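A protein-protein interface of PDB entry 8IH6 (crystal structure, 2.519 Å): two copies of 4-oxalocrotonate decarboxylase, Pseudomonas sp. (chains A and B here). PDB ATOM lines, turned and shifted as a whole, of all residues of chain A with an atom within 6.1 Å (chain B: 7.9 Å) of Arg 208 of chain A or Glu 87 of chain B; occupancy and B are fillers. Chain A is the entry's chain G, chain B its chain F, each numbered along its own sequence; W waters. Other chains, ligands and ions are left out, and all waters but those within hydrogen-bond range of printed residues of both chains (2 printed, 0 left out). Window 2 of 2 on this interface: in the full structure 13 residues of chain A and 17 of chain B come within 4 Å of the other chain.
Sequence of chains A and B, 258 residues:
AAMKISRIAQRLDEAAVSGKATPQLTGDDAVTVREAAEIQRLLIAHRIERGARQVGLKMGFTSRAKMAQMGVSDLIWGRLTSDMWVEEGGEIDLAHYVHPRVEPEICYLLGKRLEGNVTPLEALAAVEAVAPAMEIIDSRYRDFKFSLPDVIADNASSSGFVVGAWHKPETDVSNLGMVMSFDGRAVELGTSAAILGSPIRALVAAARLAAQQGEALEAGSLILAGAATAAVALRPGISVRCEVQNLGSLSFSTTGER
Asn 117 of chain A touches Trp 85 of chain B. Trp 85 of chain B touches Val 118 of chain A. Gly 89 of chain B touches Arg 201 of chain A (CA to NH2, 3.7 Å). Arg 201 of chain A touches Ser 251 of chain B (NH2 to OG, 3.5 Å). CG1 of Val 204 of chain A touches CG of Glu 87 of chain B (3.9 Å).
Water W2 lies within hydrogen-bond range of the guanidinium group of Arg 208 of chain A (3.1 Å) and the side-chain carboxylate of Glu 87 of chain B (3.5 Å). Water W1 bridges the backbone NH of Glu 88 of chain B (3.1 Å) and the backbone carbonyl oxygen of Val 118 of chain A (3.1 Å).
OE2 of Glu 88 of chain B lies within hydrogen-bond range of N of Ser 251 of chain B. The backbone NH (N) of Gly 89 of chain B is in hydrogen-bond range of the backbone carbonyl oxygen (O) of Ser 251 of chain B, at 2.6 Å. The guanidinium group (NH1) of Arg 208 of chain A is in salt-bridge range of the side-chain carboxylate (OD1) of Asp 74 of chain A, at 2.9 Å. N of Arg 208 of chain A lies within hydrogen-bond range of O of Gly 116 of chain A.
OE1 of Glu 87 of chain B lies within salt-bridge range of NE of Arg 208 of chain A, 3.5 Å away. The side-chain carboxylate of Glu 88 of chain B lies within salt-bridge range of the guanidinium group of Arg 201 of chain A (2.7 Å).
Gly 116 of chain A touches none of the printed residues of chain B. Of the printed residues of chain B, Asn 117 of chain A touches Trp 85 (3.4 Å). Arg 208 of chain A touches just one residue of chain B: Glu 87. Gln 212 of chain A touches none of the printed residues of chain B. Of the printed residues of chain A, Glu 87 of chain B touches Val 204 (3.9 Å) and Arg 208 (3.5 Å). Of the printed residues of chain A, Ser 251 of chain B touches Arg 201. The nearest residue of chain B that does not touch Arg 208 of chain A is Trp 85 of chain B (5.1 Å). The nearest printed residue of chain B that does not touch Arg 201 of chain A is Glu 87 of chain B (4.7 Å).
No position is printed for both chains.
Of the 15 printed residues of chain B, 5 touch a printed residue of chain A. Hydrophobic or aromatic side chains of chain B within 4 Å of the printed part of chain A: Trp 85. Printed residues of chain A that touch a printed residue of chain B: Asn 117, Val 118, Arg 201, Val 204 and Arg 208. Hydrophobic or aromatic side chains of chain A that line the printed part of chain B: Val 204. Among the printed residues, Asp or Glu carboxylates within 4 Å of a Lys or Arg side-chain nitrogen of the other chain: Arg 201 of chain A with Glu 88 of chain B (2.7 Å) and Arg 208 of chain A with Glu 87 of chain B (3.5 Å).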
ATOM      1  N   ASP A  74     -13.272   7.732 -16.933  1.00  0.00           N
ATOM      2  CA  ASP A  74     -14.698   7.967 -16.650  1.00  0.00           C
ATOM      3  C   ASP A  74     -14.875   9.312 -15.985  1.00  0.00           C
ATOM      4  O   ASP A  74     -13.907   9.874 -15.535  1.00  0.00           O
ATOM      5  CB  ASP A  74     -15.248   6.902 -15.721  1.00  0.00           C
ATOM      6  CG  ASP A  74     -16.674   6.555 -16.062  1.00  0.00           C
ATOM      7  OD1 ASP A  74     -17.152   6.970 -17.122  1.00  0.00           O
ATOM      8  OD2 ASP A  74     -17.323   5.898 -15.255  1.00  0.00           O
ATOM      9  N   LEU A  75     -16.123   9.734 -15.862  1.00  0.00           N
ATOM     10  CA  LEU A  75     -16.486  11.041 -15.288  1.00  0.00           C
ATOM     11  C   LEU A  75     -16.301  11.010 -13.779  1.00  0.00           C
ATOM     12  O   LEU A  75     -16.280   9.950 -13.191  1.00  0.00           O
ATOM     13  CB  LEU A  75     -17.962  11.271 -15.600  1.00  0.00           C
ATOM     14  CG  LEU A  75     -18.310  11.631 -17.037  1.00  0.00           C
ATOM     15  CD1 LEU A  75     -18.430  10.393 -17.891  1.00  0.00           C
ATOM     16  CD2 LEU A  75     -19.609  12.396 -17.077  1.00  0.00           C
ATOM     17  N   GLU A 115     -32.816   5.407 -12.017  1.00  0.00           N
ATOM     18  CA  GLU A 115     -31.818   4.530 -11.362  1.00  0.00           C
ATOM     19  C   GLU A 115     -31.159   3.567 -12.331  1.00  0.00           C
ATOM     20  O   GLU A 115     -31.868   2.986 -13.119  1.00  0.00           O
ATOM     21  CB  GLU A 115     -32.558   3.605 -10.392  1.00  0.00           C
ATOM     22  CG  GLU A 115     -31.676   2.812  -9.439  1.00  0.00           C
ATOM     23  CD  GLU A 115     -31.109   1.483  -9.900  1.00  0.00           C
ATOM     24  OE1 GLU A 115     -31.711   0.828 -10.740  1.00  0.00           O
ATOM     25  OE2 GLU A 115     -30.051   1.122  -9.419  1.00  0.00           O
ATOM     26  N   GLY A 116     -29.851   3.398 -12.190  1.00  0.00           N
ATOM     27  CA  GLY A 116     -29.125   2.329 -12.894  1.00  0.00           C
ATOM     28  C   GLY A 116     -28.735   2.614 -14.314  1.00  0.00           C
ATOM     29  O   GLY A 116     -28.342   3.712 -14.587  1.00  0.00           O
ATOM     30  N   ASN A 117     -28.751   1.577 -15.135  1.00  0.00           N
ATOM     31  CA  ASN A 117     -28.405   1.714 -16.561  1.00  0.00           C
ATOM     32  C   ASN A 117     -29.664   2.116 -17.300  1.00  0.00           C
ATOM     33  O   ASN A 117     -30.504   1.284 -17.511  1.00  0.00           O
ATOM     34  CB  ASN A 117     -27.861   0.428 -17.157  1.00  0.00           C
ATOM     35  CG  ASN A 117     -26.576  -0.001 -16.505  1.00  0.00           C
ATOM     36  OD1 ASN A 117     -25.941   0.771 -15.811  1.00  0.00           O
ATOM     37  ND2 ASN A 117     -26.201  -1.236 -16.724  1.00  0.00           N
ATOM     38  N   VAL A 118     -29.715   3.358 -17.769  1.00  0.00           N
ATOM     39  CA  VAL A 118     -30.912   3.915 -18.453  1.00  0.00           C
ATOM     40  C   VAL A 118     -30.587   4.401 -19.862  1.00  0.00           C
ATOM     41  O   VAL A 118     -29.519   4.895 -20.065  1.00  0.00           O
ATOM     42  CB  VAL A 118     -31.406   5.111 -17.637  1.00  0.00           C
ATOM     43  CG1 VAL A 118     -31.452   4.781 -16.166  1.00  0.00           C
ATOM     44  CG2 VAL A 118     -30.500   6.298 -17.865  1.00  0.00           C
ATOM     45  N   ARG A 201     -26.768  12.583 -22.254  1.00  0.00           N
ATOM     46  CA  ARG A 201     -25.818  11.482 -21.995  1.00  0.00           C
ATOM     47  C   ARG A 201     -25.296  11.590 -20.570  1.00  0.00           C
ATOM     48  O   ARG A 201     -24.998  10.573 -19.992  1.00  0.00           O
ATOM     49  CB  ARG A 201     -24.675  11.592 -22.995  1.00  0.00           C
ATOM     50  CG  ARG A 201     -24.976  10.982 -24.349  1.00  0.00           C
ATOM     51  CD  ARG A 201     -24.133  11.573 -25.435  1.00  0.00           C
ATOM     52  NE  ARG A 201     -24.365  10.773 -26.607  1.00  0.00           N
ATOM     53  CZ  ARG A 201     -23.729  10.919 -27.740  1.00  0.00           C
ATOM     54  NH1 ARG A 201     -22.817  11.855 -27.853  1.00  0.00           N
ATOM     55  NH2 ARG A 201     -24.004  10.139 -28.754  1.00  0.00           N
ATOM     56  N   LEU A 203     -26.975  12.769 -17.951  1.00  0.00           N
ATOM     57  CA  LEU A 203     -28.018  12.328 -17.006  1.00  0.00           C
ATOM     58  C   LEU A 203     -27.945  10.810 -16.927  1.00  0.00           C
ATOM     59  O   LEU A 203     -28.018  10.297 -15.837  1.00  0.00           O
ATOM     60  CB  LEU A 203     -29.368  12.814 -17.519  1.00  0.00           C
ATOM     61  CG  LEU A 203     -30.531  12.611 -16.561  1.00  0.00           C
ATOM     62  CD1 LEU A 203     -30.222  13.207 -15.209  1.00  0.00           C
ATOM     63  CD2 LEU A 203     -31.794  13.197 -17.132  1.00  0.00           C
ATOM     64  N   VAL A 204     -27.763  10.151 -18.064  1.00  0.00           N
ATOM     65  CA  VAL A 204     -27.607   8.677 -18.123  1.00  0.00           C
ATOM     66  C   VAL A 204     -26.422   8.305 -17.240  1.00  0.00           C
ATOM     67  O   VAL A 204     -26.552   7.441 -16.409  1.00  0.00           O
ATOM     68  CB  VAL A 204     -27.349   8.234 -19.565  1.00  0.00           C
ATOM     69  CG1 VAL A 204     -27.063   6.752 -19.672  1.00  0.00           C
ATOM     70  CG2 VAL A 204     -28.491   8.609 -20.462  1.00  0.00           C
ATOM     71  N   ALA A 205     -25.315   8.995 -17.454  1.00  0.00           N
ATOM     72  CA  ALA A 205     -24.059   8.825 -16.715  1.00  0.00           C
ATOM     73  C   ALA A 205     -24.327   8.952 -15.229  1.00  0.00           C
ATOM     74  O   ALA A 205     -23.884   8.127 -14.497  1.00  0.00           O
ATOM     75  CB  ALA A 205     -23.109   9.885 -17.162  1.00  0.00           C
ATOM     76  N   ALA A 206     -25.045   9.976 -14.817  1.00  0.00           N
ATOM     77  CA  ALA A 206     -25.313  10.131 -13.379  1.00  0.00           C
ATOM     78  C   ALA A 206     -26.061   8.910 -12.863  1.00  0.00           C
ATOM     79  O   ALA A 206     -25.745   8.454 -11.792  1.00  0.00           O
ATOM     80  CB  ALA A 206     -26.078  11.395 -13.136  1.00  0.00           C
ATOM     81  N   ALA A 207     -26.974   8.361 -13.643  1.00  0.00           N
ATOM     82  CA  ALA A 207     -27.698   7.188 -13.137  1.00  0.00           C
ATOM     83  C   ALA A 207     -26.716   6.039 -12.967  1.00  0.00           C
ATOM     84  O   ALA A 207     -26.817   5.363 -11.987  1.00  0.00           O
ATOM     85  CB  ALA A 207     -28.833   6.839 -14.050  1.00  0.00           C
ATOM     86  N   ARG A 208     -25.811   5.863 -13.914  1.00  0.00           N
ATOM     87  CA  ARG A 208     -24.782   4.802 -13.879  1.00  0.00           C
ATOM     88  C   ARG A 208     -23.898   5.011 -12.660  1.00  0.00           C
ATOM     89  O   ARG A 208     -23.732   4.093 -11.894  1.00  0.00           O
ATOM     90  CB  ARG A 208     -23.890   4.958 -15.108  1.00  0.00           C
ATOM     91  CG  ARG A 208     -23.185   3.691 -15.557  1.00  0.00           C
ATOM     92  CD  ARG A 208     -21.748   3.871 -15.983  1.00  0.00           C
ATOM     93  NE  ARG A 208     -21.563   4.997 -16.865  1.00  0.00           N
ATOM     94  CZ  ARG A 208     -20.481   5.741 -16.912  1.00  0.00           C
ATOM     95  NH1 ARG A 208     -19.459   5.479 -16.124  1.00  0.00           N
ATOM     96  NH2 ARG A 208     -20.410   6.752 -17.748  1.00  0.00           N
ATOM     97  N   LEU A 209     -23.336   6.209 -12.543  1.00  0.00           N
ATOM     98  CA  LEU A 209     -22.385   6.575 -11.472  1.00  0.00           C
ATOM     99  C   LEU A 209     -23.006   6.416 -10.098  1.00  0.00           C
ATOM    100  O   LEU A 209     -22.379   5.806  -9.258  1.00  0.00           O
ATOM    101  CB  LEU A 209     -21.911   8.004 -11.683  1.00  0.00           C
ATOM    102  CG  LEU A 209     -20.671   8.085 -12.546  1.00  0.00           C
ATOM    103  CD1 LEU A 209     -20.584   6.845 -13.401  1.00  0.00           C
ATOM    104  CD2 LEU A 209     -20.703   9.317 -13.408  1.00  0.00           C
ATOM    105  N   ALA A 210     -24.186   6.957  -9.858  1.00  0.00           N
ATOM    106  CA  ALA A 210     -24.721   6.798  -8.492  1.00  0.00           C
ATOM    107  C   ALA A 210     -25.001   5.322  -8.221  1.00  0.00           C
ATOM    108  O   ALA A 210     -24.992   4.937  -7.078  1.00  0.00           O
ATOM    109  CB  ALA A 210     -25.938   7.653  -8.286  1.00  0.00           C
ATOM    110  N   ALA A 211     -25.302   4.567  -9.265  1.00  0.00           N
ATOM    111  CA  ALA A 211     -25.642   3.143  -9.139  1.00  0.00           C
ATOM    112  C   ALA A 211     -24.397   2.383  -8.729  1.00  0.00           C
ATOM    113  O   ALA A 211     -24.505   1.398  -8.040  1.00  0.00           O
ATOM    114  CB  ALA A 211     -26.165   2.635 -10.444  1.00  0.00           C
ATOM    115  N   GLN A 212     -23.241   2.842  -9.179  1.00  0.00           N
ATOM    116  CA  GLN A 212     -21.983   2.170  -8.814  1.00  0.00           C
ATOM    117  C   GLN A 212     -21.837   2.253  -7.302  1.00  0.00           C
ATOM    118  O   GLN A 212     -21.138   1.434  -6.738  1.00  0.00           O
ATOM    119  CB  GLN A 212     -20.805   2.916  -9.413  1.00  0.00           C
ATOM    120  CG  GLN A 212     -20.847   3.024 -10.920  1.00  0.00           C
ATOM    121  CD  GLN A 212     -19.492   3.428 -11.431  1.00  0.00           C
ATOM    122  OE1 GLN A 212     -18.838   4.289 -10.866  1.00  0.00           O
ATOM    123  NE2 GLN A 212     -19.057   2.795 -12.503  1.00  0.00           N
ATOM    124  N   GLN A 213     -22.490   3.221  -6.684  1.00  0.00           N
ATOM    125  CA  GLN A 213     -22.377   3.360  -5.220  1.00  0.00           C
ATOM    126  C   GLN A 213     -23.711   2.990  -4.589  1.00  0.00           C
ATOM    127  O   GLN A 213     -23.999   3.476  -3.493  1.00  0.00           O
ATOM    128  CB  GLN A 213     -22.019   4.794  -4.870  1.00  0.00           C
ATOM    129  CG  GLN A 213     -20.550   5.091  -5.031  1.00  0.00           C
ATOM    130  CD  GLN A 213     -20.198   6.304  -4.216  1.00  0.00           C
ATOM    131  OE1 GLN A 213     -21.038   6.872  -3.536  1.00  0.00           O
ATOM    132  NE2 GLN A 213     -18.950   6.715  -4.289  1.00  0.00           N
ATOM    133  N   MET B  84     -27.992  -6.811 -22.048  1.00  0.00           N
ATOM    134  CA  MET B  84     -27.913  -6.469 -23.490  1.00  0.00           C
ATOM    135  C   MET B  84     -27.792  -4.955 -23.693  1.00  0.00           C
ATOM    136  O   MET B  84     -27.379  -4.546 -24.763  1.00  0.00           O
ATOM    137  CB  MET B  84     -29.179  -6.944 -24.195  1.00  0.00           C
ATOM    138  CG  MET B  84     -29.185  -8.389 -24.537  1.00  0.00           C
ATOM    139  SD  MET B  84     -30.839  -8.940 -24.346  1.00  0.00           S
ATOM    140  CE  MET B  84     -31.172  -9.720 -25.912  1.00  0.00           C
ATOM    141  N   TRP B  85     -28.149  -4.170 -22.687  1.00  0.00           N
ATOM    142  CA  TRP B  85     -28.098  -2.689 -22.761  1.00  0.00           C
ATOM    143  C   TRP B  85     -26.689  -2.179 -23.037  1.00  0.00           C
ATOM    144  O   TRP B  85     -25.771  -2.661 -22.436  1.00  0.00           O
ATOM    145  CB  TRP B  85     -28.606  -2.092 -21.453  1.00  0.00           C
ATOM    146  CG  TRP B  85     -28.446  -0.614 -21.286  1.00  0.00           C
ATOM    147  CD1 TRP B  85     -29.357   0.329 -21.623  1.00  0.00           C
ATOM    148  CD2 TRP B  85     -27.363   0.096 -20.669  1.00  0.00           C
ATOM    149  NE1 TRP B  85     -28.907   1.570 -21.296  1.00  0.00           N
ATOM    150  CE2 TRP B  85     -27.688   1.461 -20.706  1.00  0.00           C
ATOM    151  CE3 TRP B  85     -26.147  -0.274 -20.104  1.00  0.00           C
ATOM    152  CZ2 TRP B  85     -26.857   2.445 -20.194  1.00  0.00           C
ATOM    153  CZ3 TRP B  85     -25.319   0.701 -19.609  1.00  0.00           C
ATOM    154  CH2 TRP B  85     -25.668   2.042 -19.652  1.00  0.00           C
ATOM    155  N   VAL B  86     -26.566  -1.203 -23.922  1.00  0.00           N
ATOM    156  CA  VAL B  86     -25.273  -0.524 -24.195  1.00  0.00           C
ATOM    157  C   VAL B  86     -25.551   0.967 -24.088  1.00  0.00           C
ATOM    158  O   VAL B  86     -26.530   1.386 -24.632  1.00  0.00           O
ATOM    159  CB  VAL B  86     -24.730  -0.867 -25.583  1.00  0.00           C
ATOM    160  CG1 VAL B  86     -24.879  -2.334 -25.901  1.00  0.00           C
ATOM    161  CG2 VAL B  86     -25.399  -0.033 -26.636  1.00  0.00           C
ATOM    162  N   GLU B  87     -24.715   1.709 -23.382  1.00  0.00           N
ATOM    163  CA  GLU B  87     -24.895   3.166 -23.206  1.00  0.00           C
ATOM    164  C   GLU B  87     -24.811   3.869 -24.557  1.00  0.00           C
ATOM    165  O   GLU B  87     -23.867   3.621 -25.269  1.00  0.00           O
ATOM    166  CB  GLU B  87     -23.755   3.690 -22.351  1.00  0.00           C
ATOM    167  CG  GLU B  87     -24.124   4.857 -21.495  1.00  0.00           C
ATOM    168  CD  GLU B  87     -23.047   5.212 -20.507  1.00  0.00           C
ATOM    169  OE1 GLU B  87     -22.252   4.369 -20.207  1.00  0.00           O
ATOM    170  OE2 GLU B  87     -23.029   6.326 -20.053  1.00  0.00           O
ATOM    171  N   GLU B  88     -25.776   4.723 -24.876  1.00  0.00           N
ATOM    172  CA  GLU B  88     -25.740   5.505 -26.131  1.00  0.00           C
ATOM    173  C   GLU B  88     -24.532   6.434 -26.062  1.00  0.00           C
ATOM    174  O   GLU B  88     -24.353   7.094 -25.068  1.00  0.00           O
ATOM    175  CB  GLU B  88     -27.044   6.269 -26.321  1.00  0.00           C
ATOM    176  CG  GLU B  88     -27.214   6.867 -27.698  1.00  0.00           C
ATOM    177  CD  GLU B  88     -26.472   8.148 -27.994  1.00  0.00           C
ATOM    178  OE1 GLU B  88     -26.189   8.866 -27.090  1.00  0.00           O
ATOM    179  OE2 GLU B  88     -26.211   8.404 -29.133  1.00  0.00           O
ATOM    180  N   GLY B  89     -23.701   6.415 -27.094  1.00  0.00           N
ATOM    181  CA  GLY B  89     -22.448   7.191 -27.102  1.00  0.00           C
ATOM    182  C   GLY B  89     -21.321   6.388 -26.487  1.00  0.00           C
ATOM    183  O   GLY B  89     -20.250   6.923 -26.317  1.00  0.00           O
ATOM    184  N   GLY B  90     -21.605   5.139 -26.150  1.00  0.00           N
ATOM    185  CA  GLY B  90     -20.643   4.235 -25.507  1.00  0.00           C
ATOM    186  C   GLY B  90     -19.903   3.367 -26.495  1.00  0.00           C
ATOM    187  O   GLY B  90     -20.078   3.554 -27.676  1.00  0.00           O
ATOM    188  N   GLU B  91     -19.147   2.405 -25.994  1.00  0.00           N
ATOM    189  CA  GLU B  91     -18.308   1.537 -26.847  1.00  0.00           C
ATOM    190  C   GLU B  91     -18.516   0.075 -26.480  1.00  0.00           C
ATOM    191  O   GLU B  91     -18.726  -0.206 -25.338  1.00  0.00           O
ATOM    192  CB  GLU B  91     -16.856   1.916 -26.601  1.00  0.00           C
ATOM    193  CG  GLU B  91     -15.872   1.182 -27.468  1.00  0.00           C
ATOM    194  CD  GLU B  91     -14.466   1.243 -26.916  1.00  0.00           C
ATOM    195  OE1 GLU B  91     -13.833   2.284 -27.036  1.00  0.00           O
ATOM    196  OE2 GLU B  91     -14.027   0.256 -26.355  1.00  0.00           O
ATOM    197  N   ILE B  92     -18.462  -0.807 -27.466  1.00  0.00           N
ATOM    198  CA  ILE B  92     -18.572  -2.267 -27.211  1.00  0.00           C
ATOM    199  C   ILE B  92     -17.333  -2.928 -27.810  1.00  0.00           C
ATOM    200  O   ILE B  92     -16.794  -2.382 -28.768  1.00  0.00           O
ATOM    201  CB  ILE B  92     -19.865  -2.857 -27.788  1.00  0.00           C
ATOM    202  CG1 ILE B  92     -19.949  -2.709 -29.303  1.00  0.00           C
ATOM    203  CG2 ILE B  92     -21.078  -2.291 -27.105  1.00  0.00           C
ATOM    204  CD1 ILE B  92     -21.035  -3.533 -29.912  1.00  0.00           C
ATOM    205  N   PHE B 161     -28.662  -3.721 -27.387  1.00  0.00           N
ATOM    206  CA  PHE B 161     -29.665  -2.715 -27.784  1.00  0.00           C
ATOM    207  C   PHE B 161     -29.167  -1.352 -27.343  1.00  0.00           C
ATOM    208  O   PHE B 161     -28.598  -1.248 -26.289  1.00  0.00           O
ATOM    209  CB  PHE B 161     -31.052  -3.081 -27.268  1.00  0.00           C
ATOM    210  CG  PHE B 161     -31.293  -2.787 -25.818  1.00  0.00           C
ATOM    211  CD1 PHE B 161     -31.622  -1.521 -25.401  1.00  0.00           C
ATOM    212  CD2 PHE B 161     -31.215  -3.782 -24.875  1.00  0.00           C
ATOM    213  CE1 PHE B 161     -31.833  -1.247 -24.065  1.00  0.00           C
ATOM    214  CE2 PHE B 161     -31.446  -3.510 -23.545  1.00  0.00           C
ATOM    215  CZ  PHE B 161     -31.752  -2.245 -23.139  1.00  0.00           C
ATOM    216  N   VAL B 162     -29.355  -0.360 -28.198  1.00  0.00           N
ATOM    217  CA  VAL B 162     -28.942   1.028 -27.881  1.00  0.00           C
ATOM    218  C   VAL B 162     -30.082   1.939 -28.319  1.00  0.00           C
ATOM    219  O   VAL B 162     -30.600   1.748 -29.391  1.00  0.00           O
ATOM    220  CB  VAL B 162     -27.581   1.344 -28.518  1.00  0.00           C
ATOM    221  CG1 VAL B 162     -27.551   1.030 -29.993  1.00  0.00           C
ATOM    222  CG2 VAL B 162     -27.104   2.739 -28.220  1.00  0.00           C
ATOM    223  N   VAL B 163     -30.468   2.893 -27.481  1.00  0.00           N
ATOM    224  CA  VAL B 163     -31.646   3.753 -27.793  1.00  0.00           C
ATOM    225  C   VAL B 163     -31.254   5.231 -27.861  1.00  0.00           C
ATOM    226  O   VAL B 163     -30.371   5.636 -27.150  1.00  0.00           O
ATOM    227  CB  VAL B 163     -32.769   3.484 -26.770  1.00  0.00           C
ATOM    228  CG1 VAL B 163     -34.093   4.127 -27.105  1.00  0.00           C
ATOM    229  CG2 VAL B 163     -32.993   2.006 -26.591  1.00  0.00           C
ATOM    230  N   SER B 251     -25.734   6.790 -31.375  1.00  0.00           N
ATOM    231  CA  SER B 251     -24.479   6.154 -31.832  1.00  0.00           C
ATOM    232  C   SER B 251     -23.770   5.415 -30.707  1.00  0.00           C
ATOM    233  O   SER B 251     -24.125   5.551 -29.561  1.00  0.00           O
ATOM    234  CB  SER B 251     -23.565   7.150 -32.452  1.00  0.00           C
ATOM    235  OG  SER B 251     -23.206   8.124 -31.517  1.00  0.00           O
ATOM    236  N   PHE B 252     -22.805   4.617 -31.105  1.00  0.00           N
ATOM    237  CA  PHE B 252     -21.933   3.825 -30.220  1.00  0.00           C
ATOM    238  C   PHE B 252     -20.723   3.446 -31.058  1.00  0.00           C
ATOM    239  O   PHE B 252     -20.822   3.348 -32.260  1.00  0.00           O
ATOM    240  CB  PHE B 252     -22.666   2.599 -29.692  1.00  0.00           C
ATOM    241  CG  PHE B 252     -22.940   1.547 -30.725  1.00  0.00           C
ATOM    242  CD1 PHE B 252     -24.096   1.572 -31.467  1.00  0.00           C
ATOM    243  CD2 PHE B 252     -22.041   0.531 -30.939  1.00  0.00           C
ATOM    244  CE1 PHE B 252     -24.350   0.598 -32.408  1.00  0.00           C
ATOM    245  CE2 PHE B 252     -22.297  -0.443 -31.877  1.00  0.00           C
ATOM    246  CZ  PHE B 252     -23.452  -0.414 -32.603  1.00  0.00           C
ATOM    247  N   SER B 253     -19.581   3.264 -30.417  1.00  0.00           N
ATOM    248  CA  SER B 253     -18.389   2.924 -31.214  1.00  0.00           C
ATOM    249  C   SER B 253     -17.935   1.516 -30.882  1.00  0.00           C
ATOM    250  O   SER B 253     -18.352   0.999 -29.860  1.00  0.00           O
ATOM    251  CB  SER B 253     -17.310   3.908 -30.977  1.00  0.00           C
ATOM    252  OG  SER B 253     -16.686   3.649 -29.745  1.00  0.00           O
HETATM  253  O   HOH W   1     -27.920   5.293 -22.734  1.00  0.00           O
HETATM  254  O   HOH W   2     -20.070   8.092 -20.503  1.00  0.00           O
